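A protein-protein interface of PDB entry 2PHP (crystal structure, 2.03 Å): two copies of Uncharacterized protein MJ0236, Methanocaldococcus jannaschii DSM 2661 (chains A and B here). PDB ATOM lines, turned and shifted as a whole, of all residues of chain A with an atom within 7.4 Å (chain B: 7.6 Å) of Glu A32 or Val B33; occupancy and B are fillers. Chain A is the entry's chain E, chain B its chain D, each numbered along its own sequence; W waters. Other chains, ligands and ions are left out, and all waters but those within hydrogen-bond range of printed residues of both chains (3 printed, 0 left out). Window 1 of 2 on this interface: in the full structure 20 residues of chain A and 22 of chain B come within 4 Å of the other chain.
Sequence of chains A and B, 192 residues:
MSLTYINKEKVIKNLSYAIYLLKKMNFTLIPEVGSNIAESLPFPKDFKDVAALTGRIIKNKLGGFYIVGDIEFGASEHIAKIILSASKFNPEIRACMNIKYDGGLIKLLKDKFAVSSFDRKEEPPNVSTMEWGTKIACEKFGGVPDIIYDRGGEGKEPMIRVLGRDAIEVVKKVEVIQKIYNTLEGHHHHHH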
ATOM      1  N   ILE A  30     -19.756  20.495  17.966  1.00  0.00           N
ATOM      2  CA  ILE A  30     -21.116  20.028  17.783  1.00  0.00           C
ATOM      3  C   ILE A  30     -21.728  19.573  19.096  1.00  0.00           C
ATOM      4  O   ILE A  30     -21.161  18.743  19.801  1.00  0.00           O
ATOM      5  CB  ILE A  30     -21.142  18.864  16.774  1.00  0.00           C
ATOM      6  CG1 ILE A  30     -20.410  19.290  15.498  1.00  0.00           C
ATOM      7  CG2 ILE A  30     -22.583  18.452  16.470  1.00  0.00           C
ATOM      8  CD1 ILE A  30     -20.311  18.207  14.450  1.00  0.00           C
ATOM      9  N   PRO A  31     -22.898  20.121  19.450  1.00  0.00           N
ATOM     10  CA  PRO A  31     -23.550  19.728  20.700  1.00  0.00           C
ATOM     11  C   PRO A  31     -24.254  18.377  20.553  1.00  0.00           C
ATOM     12  O   PRO A  31     -24.465  17.884  19.435  1.00  0.00           O
ATOM     13  CB  PRO A  31     -24.543  20.859  20.931  1.00  0.00           C
ATOM     14  CG  PRO A  31     -24.996  21.152  19.549  1.00  0.00           C
ATOM     15  CD  PRO A  31     -23.680  21.165  18.764  1.00  0.00           C
ATOM     16  N   GLU A  32     -24.623  17.792  21.685  1.00  0.00           N
ATOM     17  CA  GLU A  32     -25.319  16.513  21.699  1.00  0.00           C
ATOM     18  C   GLU A  32     -26.598  16.550  20.849  1.00  0.00           C
ATOM     19  O   GLU A  32     -27.001  15.529  20.293  1.00  0.00           O
ATOM     20  CB  GLU A  32     -25.659  16.121  23.143  1.00  0.00           C
ATOM     21  CG  GLU A  32     -24.435  16.000  24.054  1.00  0.00           C
ATOM     22  CD  GLU A  32     -24.791  16.034  25.548  1.00  0.00           C
ATOM     23  OE1 GLU A  32     -25.557  15.154  26.016  1.00  0.00           O
ATOM     24  OE2 GLU A  32     -24.301  16.944  26.255  1.00  0.00           O
ATOM     25  N   VAL A  33     -27.234  17.716  20.750  1.00  0.00           N
ATOM     26  CA  VAL A  33     -28.458  17.834  19.953  1.00  0.00           C
ATOM     27  C   VAL A  33     -28.153  18.197  18.500  1.00  0.00           C
ATOM     28  O   VAL A  33     -29.066  18.421  17.703  1.00  0.00           O
ATOM     29  CB  VAL A  33     -29.428  18.911  20.524  1.00  0.00           C
ATOM     30  CG1 VAL A  33     -29.833  18.547  21.942  1.00  0.00           C
ATOM     31  CG2 VAL A  33     -28.778  20.289  20.477  1.00  0.00           C
ATOM     32  N   GLY A  34     -26.867  18.268  18.165  1.00  0.00           N
ATOM     33  CA  GLY A  34     -26.476  18.595  16.805  1.00  0.00           C
ATOM     34  C   GLY A  34     -26.608  20.060  16.444  1.00  0.00           C
ATOM     35  O   GLY A  34     -27.356  20.805  17.082  1.00  0.00           O
ATOM     36  N   SER A  35     -25.878  20.477  15.414  1.00  0.00           N
ATOM     37  CA  SER A  35     -25.905  21.868  14.959  1.00  0.00           C
ATOM     38  C   SER A  35     -26.736  22.060  13.700  1.00  0.00           C
ATOM     39  O   SER A  35     -26.889  21.142  12.896  1.00  0.00           O
ATOM     40  CB  SER A  35     -24.484  22.365  14.647  1.00  0.00           C
ATOM     41  OG  SER A  35     -23.663  22.430  15.801  1.00  0.00           O
ATOM     42  N   ARG A  56     -29.649  17.864  10.438  1.00  0.00           N
ATOM     43  CA  ARG A  56     -28.817  18.549  11.418  1.00  0.00           C
ATOM     44  C   ARG A  56     -27.377  18.170  11.099  1.00  0.00           C
ATOM     45  O   ARG A  56     -27.124  17.376  10.191  1.00  0.00           O
ATOM     46  CB  ARG A  56     -29.157  18.086  12.841  1.00  0.00           C
ATOM     47  CG  ARG A  56     -29.202  19.202  13.885  1.00  0.00           C
ATOM     48  CD  ARG A  56     -30.637  19.679  14.124  1.00  0.00           C
ATOM     49  NE  ARG A  56     -30.716  21.064  14.602  1.00  0.00           N
ATOM     50  CZ  ARG A  56     -30.455  21.482  15.845  1.00  0.00           C
ATOM     51  NH1 ARG A  56     -30.089  20.626  16.791  1.00  0.00           N
ATOM     52  NH2 ARG A  56     -30.559  22.779  16.146  1.00  0.00           N
ATOM     53  N   ILE A  57     -26.440  18.759  11.828  1.00  0.00           N
ATOM     54  CA  ILE A  57     -25.035  18.448  11.662  1.00  0.00           C
ATOM     55  C   ILE A  57     -24.690  17.695  12.943  1.00  0.00           C
ATOM     56  O   ILE A  57     -24.862  18.223  14.050  1.00  0.00           O
ATOM     57  CB  ILE A  57     -24.197  19.740  11.527  1.00  0.00           C
ATOM     58  CG1 ILE A  57     -24.609  20.474  10.244  1.00  0.00           C
ATOM     59  CG2 ILE A  57     -22.714  19.403  11.482  1.00  0.00           C
ATOM     60  CD1 ILE A  57     -24.079  21.883  10.137  1.00  0.00           C
ATOM     61  N   ILE A  58     -24.257  16.445  12.795  1.00  0.00           N
ATOM     62  CA  ILE A  58     -23.919  15.608  13.942  1.00  0.00           C
ATOM     63  C   ILE A  58     -22.522  15.024  13.814  1.00  0.00           C
ATOM     64  O   ILE A  58     -21.963  14.954  12.722  1.00  0.00           O
ATOM     65  CB  ILE A  58     -24.909  14.426  14.095  1.00  0.00           C
ATOM     66  CG1 ILE A  58     -24.861  13.544  12.843  1.00  0.00           C
ATOM     67  CG2 ILE A  58     -26.335  14.946  14.351  1.00  0.00           C
ATOM     68  CD1 ILE A  58     -25.738  12.308  12.932  1.00  0.00           C
ATOM     69  N   LYS A  59     -21.953  14.612  14.938  1.00  0.00           N
ATOM     70  CA  LYS A  59     -20.618  14.030  14.926  1.00  0.00           C
ATOM     71  C   LYS A  59     -20.591  12.638  14.302  1.00  0.00           C
ATOM     72  O   LYS A  59     -21.570  11.890  14.348  1.00  0.00           O
ATOM     73  CB  LYS A  59     -20.054  13.915  16.345  1.00  0.00           C
ATOM     74  CG  LYS A  59     -19.509  15.197  16.920  1.00  0.00           C
ATOM     75  CD  LYS A  59     -18.911  14.963  18.299  1.00  0.00           C
ATOM     76  CE  LYS A  59     -18.401  16.276  18.881  1.00  0.00           C
ATOM     77  NZ  LYS A  59     -17.738  16.100  20.201  1.00  0.00           N
ATOM     78  N   LYS A 100     -21.544  23.861  20.050  1.00  0.00           N
ATOM     79  CA  LYS A 100     -21.255  23.362  21.387  1.00  0.00           C
ATOM     80  C   LYS A 100     -20.728  24.466  22.310  1.00  0.00           C
ATOM     81  O   LYS A 100     -20.028  25.385  21.871  1.00  0.00           O
ATOM     82  CB  LYS A 100     -20.225  22.240  21.286  1.00  0.00           C
ATOM     83  CG  LYS A 100     -19.866  21.561  22.594  1.00  0.00           C
ATOM     84  CD  LYS A 100     -18.785  20.533  22.324  1.00  0.00           C
ATOM     85  CE  LYS A 100     -18.393  19.756  23.560  1.00  0.00           C
ATOM     86  NZ  LYS A 100     -17.348  18.749  23.192  1.00  0.00           N
ATOM     87  N   GLU A 157     -29.054  21.298  27.273  1.00  0.00           N
ATOM     88  CA  GLU A 157     -27.609  21.441  27.359  1.00  0.00           C
ATOM     89  C   GLU A 157     -27.210  22.885  27.074  1.00  0.00           C
ATOM     90  O   GLU A 157     -27.938  23.610  26.397  1.00  0.00           O
ATOM     91  CB  GLU A 157     -26.913  20.484  26.386  1.00  0.00           C
ATOM     92  CG  GLU A 157     -27.049  20.836  24.915  1.00  0.00           C
ATOM     93  CD  GLU A 157     -26.469  19.757  24.003  1.00  0.00           C
ATOM     94  OE1 GLU A 157     -27.263  19.116  23.281  1.00  0.00           O
ATOM     95  OE2 GLU A 157     -25.229  19.546  24.011  1.00  0.00           O
ATOM     96  N   PRO A 158     -26.053  23.326  27.602  1.00  0.00           N
ATOM     97  CA  PRO A 158     -25.598  24.701  27.373  1.00  0.00           C
ATOM     98  C   PRO A 158     -25.436  24.894  25.867  1.00  0.00           C
ATOM     99  O   PRO A 158     -25.348  23.907  25.125  1.00  0.00           O
ATOM    100  CB  PRO A 158     -24.252  24.754  28.095  1.00  0.00           C
ATOM    101  CG  PRO A 158     -24.326  23.640  29.091  1.00  0.00           C
ATOM    102  CD  PRO A 158     -25.033  22.558  28.336  1.00  0.00           C
ATOM    103  N   MET A 159     -25.385  26.142  25.413  1.00  0.00           N
ATOM    104  CA  MET A 159     -25.245  26.393  23.983  1.00  0.00           C
ATOM    105  C   MET A 159     -24.641  27.747  23.651  1.00  0.00           C
ATOM    106  O   MET A 159     -24.818  28.726  24.381  1.00  0.00           O
ATOM    107  CB  MET A 159     -26.612  26.296  23.299  1.00  0.00           C
ATOM    108  CG  MET A 159     -26.547  26.099  21.792  1.00  0.00           C
ATOM    109  SD  MET A 159     -25.944  24.293  21.356  1.00  0.00           S
ATOM    110  CE  MET A 159     -27.451  23.312  22.082  1.00  0.00           C
ATOM    111  N   ILE B  30     -38.313   9.913  18.812  1.00  0.00           N
ATOM    112  CA  ILE B  30     -36.938  10.358  18.631  1.00  0.00           C
ATOM    113  C   ILE B  30     -36.566  11.550  19.539  1.00  0.00           C
ATOM    114  O   ILE B  30     -37.168  12.625  19.448  1.00  0.00           O
ATOM    115  CB  ILE B  30     -36.699  10.787  17.172  1.00  0.00           C
ATOM    116  CG1 ILE B  30     -37.149   9.692  16.200  1.00  0.00           C
ATOM    117  CG2 ILE B  30     -35.235  11.083  16.969  1.00  0.00           C
ATOM    118  CD1 ILE B  30     -37.001  10.090  14.725  1.00  0.00           C
ATOM    119  N   PRO B  31     -35.588  11.366  20.440  1.00  0.00           N
ATOM    120  CA  PRO B  31     -35.156  12.443  21.337  1.00  0.00           C
ATOM    121  C   PRO B  31     -34.346  13.483  20.582  1.00  0.00           C
ATOM    122  O   PRO B  31     -33.753  13.186  19.543  1.00  0.00           O
ATOM    123  CB  PRO B  31     -34.313  11.710  22.378  1.00  0.00           C
ATOM    124  CG  PRO B  31     -33.798  10.517  21.610  1.00  0.00           C
ATOM    125  CD  PRO B  31     -35.052  10.081  20.907  1.00  0.00           C
ATOM    126  N   GLU B  32     -34.307  14.697  21.113  1.00  0.00           N
ATOM    127  CA  GLU B  32     -33.569  15.767  20.473  1.00  0.00           C
ATOM    128  C   GLU B  32     -32.091  15.454  20.299  1.00  0.00           C
ATOM    129  O   GLU B  32     -31.431  16.050  19.449  1.00  0.00           O
ATOM    130  CB  GLU B  32     -33.771  17.069  21.250  1.00  0.00           C
ATOM    131  CG  GLU B  32     -35.129  17.703  20.961  1.00  0.00           C
ATOM    132  CD  GLU B  32     -35.762  18.338  22.190  1.00  0.00           C
ATOM    133  OE1 GLU B  32     -35.191  19.317  22.721  1.00  0.00           O
ATOM    134  OE2 GLU B  32     -36.833  17.854  22.625  1.00  0.00           O
ATOM    135  N   VAL B  33     -31.567  14.514  21.086  1.00  0.00           N
ATOM    136  CA  VAL B  33     -30.151  14.142  20.957  1.00  0.00           C
ATOM    137  C   VAL B  33     -29.952  12.987  19.969  1.00  0.00           C
ATOM    138  O   VAL B  33     -28.830  12.531  19.749  1.00  0.00           O
ATOM    139  CB  VAL B  33     -29.522  13.721  22.314  1.00  0.00           C
ATOM    140  CG1 VAL B  33     -29.472  14.915  23.259  1.00  0.00           C
ATOM    141  CG2 VAL B  33     -30.309  12.573  22.931  1.00  0.00           C
ATOM    142  N   GLY B  34     -31.054  12.533  19.381  1.00  0.00           N
ATOM    143  CA  GLY B  34     -31.010  11.435  18.432  1.00  0.00           C
ATOM    144  C   GLY B  34     -30.951  10.083  19.127  1.00  0.00           C
ATOM    145  O   GLY B  34     -30.575   9.979  20.297  1.00  0.00           O
ATOM    146  N   SER B  35     -31.317   9.040  18.397  1.00  0.00           N
ATOM    147  CA  SER B  35     -31.283   7.687  18.924  1.00  0.00           C
ATOM    148  C   SER B  35     -30.185   6.893  18.256  1.00  0.00           C
ATOM    149  O   SER B  35     -29.802   7.177  17.119  1.00  0.00           O
ATOM    150  CB  SER B  35     -32.598   6.964  18.654  1.00  0.00           C
ATOM    151  OG  SER B  35     -33.649   7.509  19.421  1.00  0.00           O
ATOM    152  N   ASN B  36     -29.677   5.896  18.968  1.00  0.00           N
ATOM    153  CA  ASN B  36     -28.680   5.014  18.408  1.00  0.00           C
ATOM    154  C   ASN B  36     -29.057   3.642  18.915  1.00  0.00           C
ATOM    155  O   ASN B  36     -29.812   3.522  19.878  1.00  0.00           O
ATOM    156  CB  ASN B  36     -27.270   5.371  18.863  1.00  0.00           C
ATOM    157  CG  ASN B  36     -26.212   4.811  17.914  1.00  0.00           C
ATOM    158  OD1 ASN B  36     -26.511   3.940  17.081  1.00  0.00           O
ATOM    159  ND2 ASN B  36     -24.981   5.299  18.031  1.00  0.00           N
ATOM    160  N   GLY B  55     -23.285   7.471  13.208  1.00  0.00           N
ATOM    161  CA  GLY B  55     -24.044   8.705  13.281  1.00  0.00           C
ATOM    162  C   GLY B  55     -25.130   8.505  14.321  1.00  0.00           C
ATOM    163  O   GLY B  55     -24.846   8.127  15.451  1.00  0.00           O
ATOM    164  N   ARG B  56     -26.376   8.748  13.944  1.00  0.00           N
ATOM    165  CA  ARG B  56     -27.497   8.569  14.851  1.00  0.00           C
ATOM    166  C   ARG B  56     -28.778   8.609  14.041  1.00  0.00           C
ATOM    167  O   ARG B  56     -28.747   8.835  12.838  1.00  0.00           O
ATOM    168  CB  ARG B  56     -27.508   9.662  15.930  1.00  0.00           C
ATOM    169  CG  ARG B  56     -27.394   9.100  17.353  1.00  0.00           C
ATOM    170  CD  ARG B  56     -26.573   9.981  18.295  1.00  0.00           C
ATOM    171  NE  ARG B  56     -26.127   9.221  19.465  1.00  0.00           N
ATOM    172  CZ  ARG B  56     -26.883   8.951  20.530  1.00  0.00           C
ATOM    173  NH1 ARG B  56     -28.136   9.388  20.594  1.00  0.00           N
ATOM    174  NH2 ARG B  56     -26.399   8.213  21.524  1.00  0.00           N
ATOM    175  N   ILE B  57     -29.901   8.342  14.689  1.00  0.00           N
ATOM    176  CA  ILE B  57     -31.184   8.382  14.011  1.00  0.00           C
ATOM    177  C   ILE B  57     -31.798   9.697  14.469  1.00  0.00           C
ATOM    178  O   ILE B  57     -32.082   9.869  15.651  1.00  0.00           O
ATOM    179  CB  ILE B  57     -32.060   7.190  14.430  1.00  0.00           C
ATOM    180  CG1 ILE B  57     -31.364   5.890  14.018  1.00  0.00           C
ATOM    181  CG2 ILE B  57     -33.429   7.277  13.781  1.00  0.00           C
ATOM    182  CD1 ILE B  57     -31.971   4.648  14.651  1.00  0.00           C
ATOM    183  N   ILE B  58     -31.958  10.638  13.540  1.00  0.00           N
ATOM    184  CA  ILE B  58     -32.507  11.946  13.878  1.00  0.00           C
ATOM    185  C   ILE B  58     -33.762  12.275  13.081  1.00  0.00           C
ATOM    186  O   ILE B  58     -34.031  11.667  12.043  1.00  0.00           O
ATOM    187  CB  ILE B  58     -31.468  13.066  13.634  1.00  0.00           C
ATOM    188  CG1 ILE B  58     -31.182  13.205  12.134  1.00  0.00           C
ATOM    189  CG2 ILE B  58     -30.172  12.753  14.390  1.00  0.00           C
ATOM    190  CD1 ILE B  58     -30.284  14.383  11.788  1.00  0.00           C
ATOM    191  N   HIS B  78     -21.009   5.723  24.739  1.00  0.00           N
ATOM    192  CA  HIS B  78     -22.182   5.998  25.556  1.00  0.00           C
ATOM    193  C   HIS B  78     -22.986   4.717  25.742  1.00  0.00           C
ATOM    194  O   HIS B  78     -22.982   4.149  26.830  1.00  0.00           O
ATOM    195  CB  HIS B  78     -23.054   7.080  24.900  1.00  0.00           C
ATOM    196  CG  HIS B  78     -24.243   7.484  25.717  1.00  0.00           C
ATOM    197  ND1 HIS B  78     -24.136   8.212  26.885  1.00  0.00           N
ATOM    198  CD2 HIS B  78     -25.566   7.255  25.539  1.00  0.00           C
ATOM    199  CE1 HIS B  78     -25.342   8.413  27.389  1.00  0.00           C
ATOM    200  NE2 HIS B  78     -26.228   7.842  26.590  1.00  0.00           N
ATOM    201  N   ASN B  98     -31.730   3.820  22.692  1.00  0.00           N
ATOM    202  CA  ASN B  98     -32.348   4.878  23.481  1.00  0.00           C
ATOM    203  C   ASN B  98     -33.427   5.585  22.667  1.00  0.00           C
ATOM    204  O   ASN B  98     -33.207   5.958  21.511  1.00  0.00           O
ATOM    205  CB  ASN B  98     -31.305   5.895  23.955  1.00  0.00           C
ATOM    206  CG  ASN B  98     -30.769   6.762  22.831  1.00  0.00           C
ATOM    207  OD1 ASN B  98     -30.012   6.302  21.978  1.00  0.00           O
ATOM    208  ND2 ASN B  98     -31.160   8.032  22.828  1.00  0.00           N
ATOM    209  N   ARG B 120     -30.397  10.993  38.092  1.00  0.00           N
ATOM    210  CA  ARG B 120     -29.136  11.670  37.841  1.00  0.00           C
ATOM    211  C   ARG B 120     -28.563  12.483  39.001  1.00  0.00           C
ATOM    212  O   ARG B 120     -27.348  12.651  39.092  1.00  0.00           O
ATOM    213  CB  ARG B 120     -29.265  12.557  36.598  1.00  0.00           C
ATOM    214  CG  ARG B 120     -29.372  11.769  35.283  1.00  0.00           C
ATOM    215  CD  ARG B 120     -29.498  12.697  34.083  1.00  0.00           C
ATOM    216  NE  ARG B 120     -29.354  11.990  32.813  1.00  0.00           N
ATOM    217  CZ  ARG B 120     -28.185  11.684  32.257  1.00  0.00           C
ATOM    218  NH1 ARG B 120     -27.049  12.023  32.852  1.00  0.00           N
ATOM    219  NH2 ARG B 120     -28.144  11.032  31.101  1.00  0.00           N
ATOM    220  N   GLY B 155     -28.872  19.960  32.092  1.00  0.00           N
ATOM    221  CA  GLY B 155     -28.242  19.775  30.793  1.00  0.00           C
ATOM    222  C   GLY B 155     -28.444  18.400  30.173  1.00  0.00           C
ATOM    223  O   GLY B 155     -27.746  18.035  29.226  1.00  0.00           O
ATOM    224  N   LYS B 156     -29.399  17.636  30.697  1.00  0.00           N
ATOM    225  CA  LYS B 156     -29.664  16.291  30.191  1.00  0.00           C
ATOM    226  C   LYS B 156     -31.144  16.017  29.971  1.00  0.00           C
ATOM    227  O   LYS B 156     -31.961  16.124  30.887  1.00  0.00           O
ATOM    228  CB  LYS B 156     -29.111  15.240  31.157  1.00  0.00           C
ATOM    229  CG  LYS B 156     -27.605  15.276  31.350  1.00  0.00           C
ATOM    230  CD  LYS B 156     -26.871  14.846  30.092  1.00  0.00           C
ATOM    231  CE  LYS B 156     -25.380  14.717  30.349  1.00  0.00           C
ATOM    232  NZ  LYS B 156     -24.657  14.302  29.125  1.00  0.00           N
ATOM    233  N   GLU B 157     -31.474  15.638  28.745  1.00  0.00           N
ATOM    234  CA  GLU B 157     -32.841  15.326  28.363  1.00  0.00           C
ATOM    235  C   GLU B 157     -33.262  13.971  28.949  1.00  0.00           C
ATOM    236  O   GLU B 157     -32.435  13.070  29.091  1.00  0.00           O
ATOM    237  CB  GLU B 157     -32.919  15.308  26.829  1.00  0.00           C
ATOM    238  CG  GLU B 157     -34.048  14.489  26.222  1.00  0.00           C
ATOM    239  CD  GLU B 157     -34.090  14.599  24.697  1.00  0.00           C
ATOM    240  OE1 GLU B 157     -33.012  14.516  24.057  1.00  0.00           O
ATOM    241  OE2 GLU B 157     -35.201  14.763  24.140  1.00  0.00           O
ATOM    242  N   PRO B 158     -34.546  13.824  29.329  1.00  0.00           N
ATOM    243  CA  PRO B 158     -35.055  12.566  29.892  1.00  0.00           C
ATOM    244  C   PRO B 158     -34.999  11.469  28.821  1.00  0.00           C
ATOM    245  O   PRO B 158     -35.243  11.738  27.643  1.00  0.00           O
ATOM    246  CB  PRO B 158     -36.483  12.924  30.297  1.00  0.00           C
ATOM    247  CG  PRO B 158     -36.848  14.018  29.329  1.00  0.00           C
ATOM    248  CD  PRO B 158     -35.600  14.853  29.315  1.00  0.00           C
ATOM    249  N   MET B 159     -34.696  10.239  29.223  1.00  0.00           N
ATOM    250  CA  MET B 159     -34.568   9.159  28.247  1.00  0.00           C
ATOM    251  C   MET B 159     -35.172   7.820  28.647  1.00  0.00           C
ATOM    252  O   MET B 159     -35.307   7.508  29.828  1.00  0.00           O
ATOM    253  CB  MET B 159     -33.083   8.938  27.944  1.00  0.00           C
ATOM    254  CG  MET B 159     -32.799   8.266  26.619  1.00  0.00           C
ATOM    255  SD  MET B 159     -33.216   9.470  25.174  1.00  0.00           S
ATOM    256  CE  MET B 159     -31.807  10.759  25.484  1.00  0.00           C
HETATM  257  O   HOH W   1     -26.119  12.694  20.234  1.00  0.00           O
HETATM  258  O   HOH W   2     -27.777  14.566  17.430  1.00  0.00           O
HETATM  259  O   HOH W   3     -30.413  15.483  16.756  1.00  0.00           O
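The side-chain amino group (NZ) of Lys B156 lies within salt-bridge range of the side-chain carboxylate (OE1) of Glu A32 (3.3 Å).
The backbone carbonyl oxygen (O) of Gly B34 is in hydrogen-bond range of the guanidinium group (NH1) of Arg B56 (2.5 Å). N of Glu B32 is in hydrogen-bond range of OE2 of Glu B157 (3.2 Å). N of Glu A32 lies within hydrogen-bond range of OE2 of Glu A157, 3.0 Å away. N of Val A33 is in hydrogen-bond range of OE1 of Glu A157, 2.9 Å away. The side-chain carboxylate (OE1) of Glu B157 sits at hydrogen-bond distance from the backbone NH (N) of Val B33, at 3.3 Å. NH1 of Arg A56 lies within hydrogen-bond range of O of Gly A34, 2.8 Å away.
O of Glu A32 touches CA of Val B33 (3.5 Å). O of Glu B32 touches CA of Val A33, at 3.5 Å. CG1 of Val A33 touches CG1 of Val B33 (3.9 Å). CD1 of Ile B58 touches N of Arg A56, 3.8 Å away. Ile A58 touches Gly B55. Arg B56 touches Ile A58. O of Gly B155 touches CB of Glu A157, 3.8 Å away.
Of chain B, only Val B33 (3.5 Å) and Lys B156 (3.3 Å) come within 4 Å of Glu A32. Lys A59 touches none of the printed residues of chain B. Val B33 touches two residues of chain A. No residue of chain A comes within 4 Å of Gly B34. Of the printed residues of chain A, Gly B55 touches Ile A58. Printed residues of chain A within 4 Å of Arg B56: Ile A58 (3.8 Å). Of the printed residues of chain A, Ile B58 touches Arg A56. Of the printed residues of chain A, Lys B156 touches Glu A32 (3.3 Å). The nearest residue of chain B that does not touch Glu A32 is Glu B32 (4.5 Å).
Printed residues of chain B that touch a printed residue of chain A: Glu B32, Val B33, Gly B55, Arg B56, Ile B58, Gly B155 and Lys B156. Hydrophobic or aromatic side chains of chain B that line the printed part of chain A: Val B33 and Ile B58. Hydrophobic or aromatic side chains of chain A that line the printed part of chain B: Val A33 and Ile A58.
Glu A32 touches Val B33, and with the chains exchanged Val A33 touches Glu B32. Val A33 touches its own counterpart, Val B33. Arg A56 touches Ile B58, and with the chains exchanged Ile A58 touches Arg B56. Positions printed for both chains: 30, 31, 32, 33, 34, 35, 56, 57, 58, 157, 158 and 159.
Water W1 lies within hydrogen-bond range of the backbone carbonyl oxygen of Val B33 (2.8 Å) and the backbone carbonyl oxygen of Glu A32 (3.0 Å). Water W3 bridges O of Glu B32 (2.9 Å) and O of Val A33 (3.4 Å). Water W2 bridges the backbone carbonyl oxygen (O) of Glu A32 (3.1 Å) and the backbone carbonyl oxygen (O) of Val B33 (3.3 Å).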
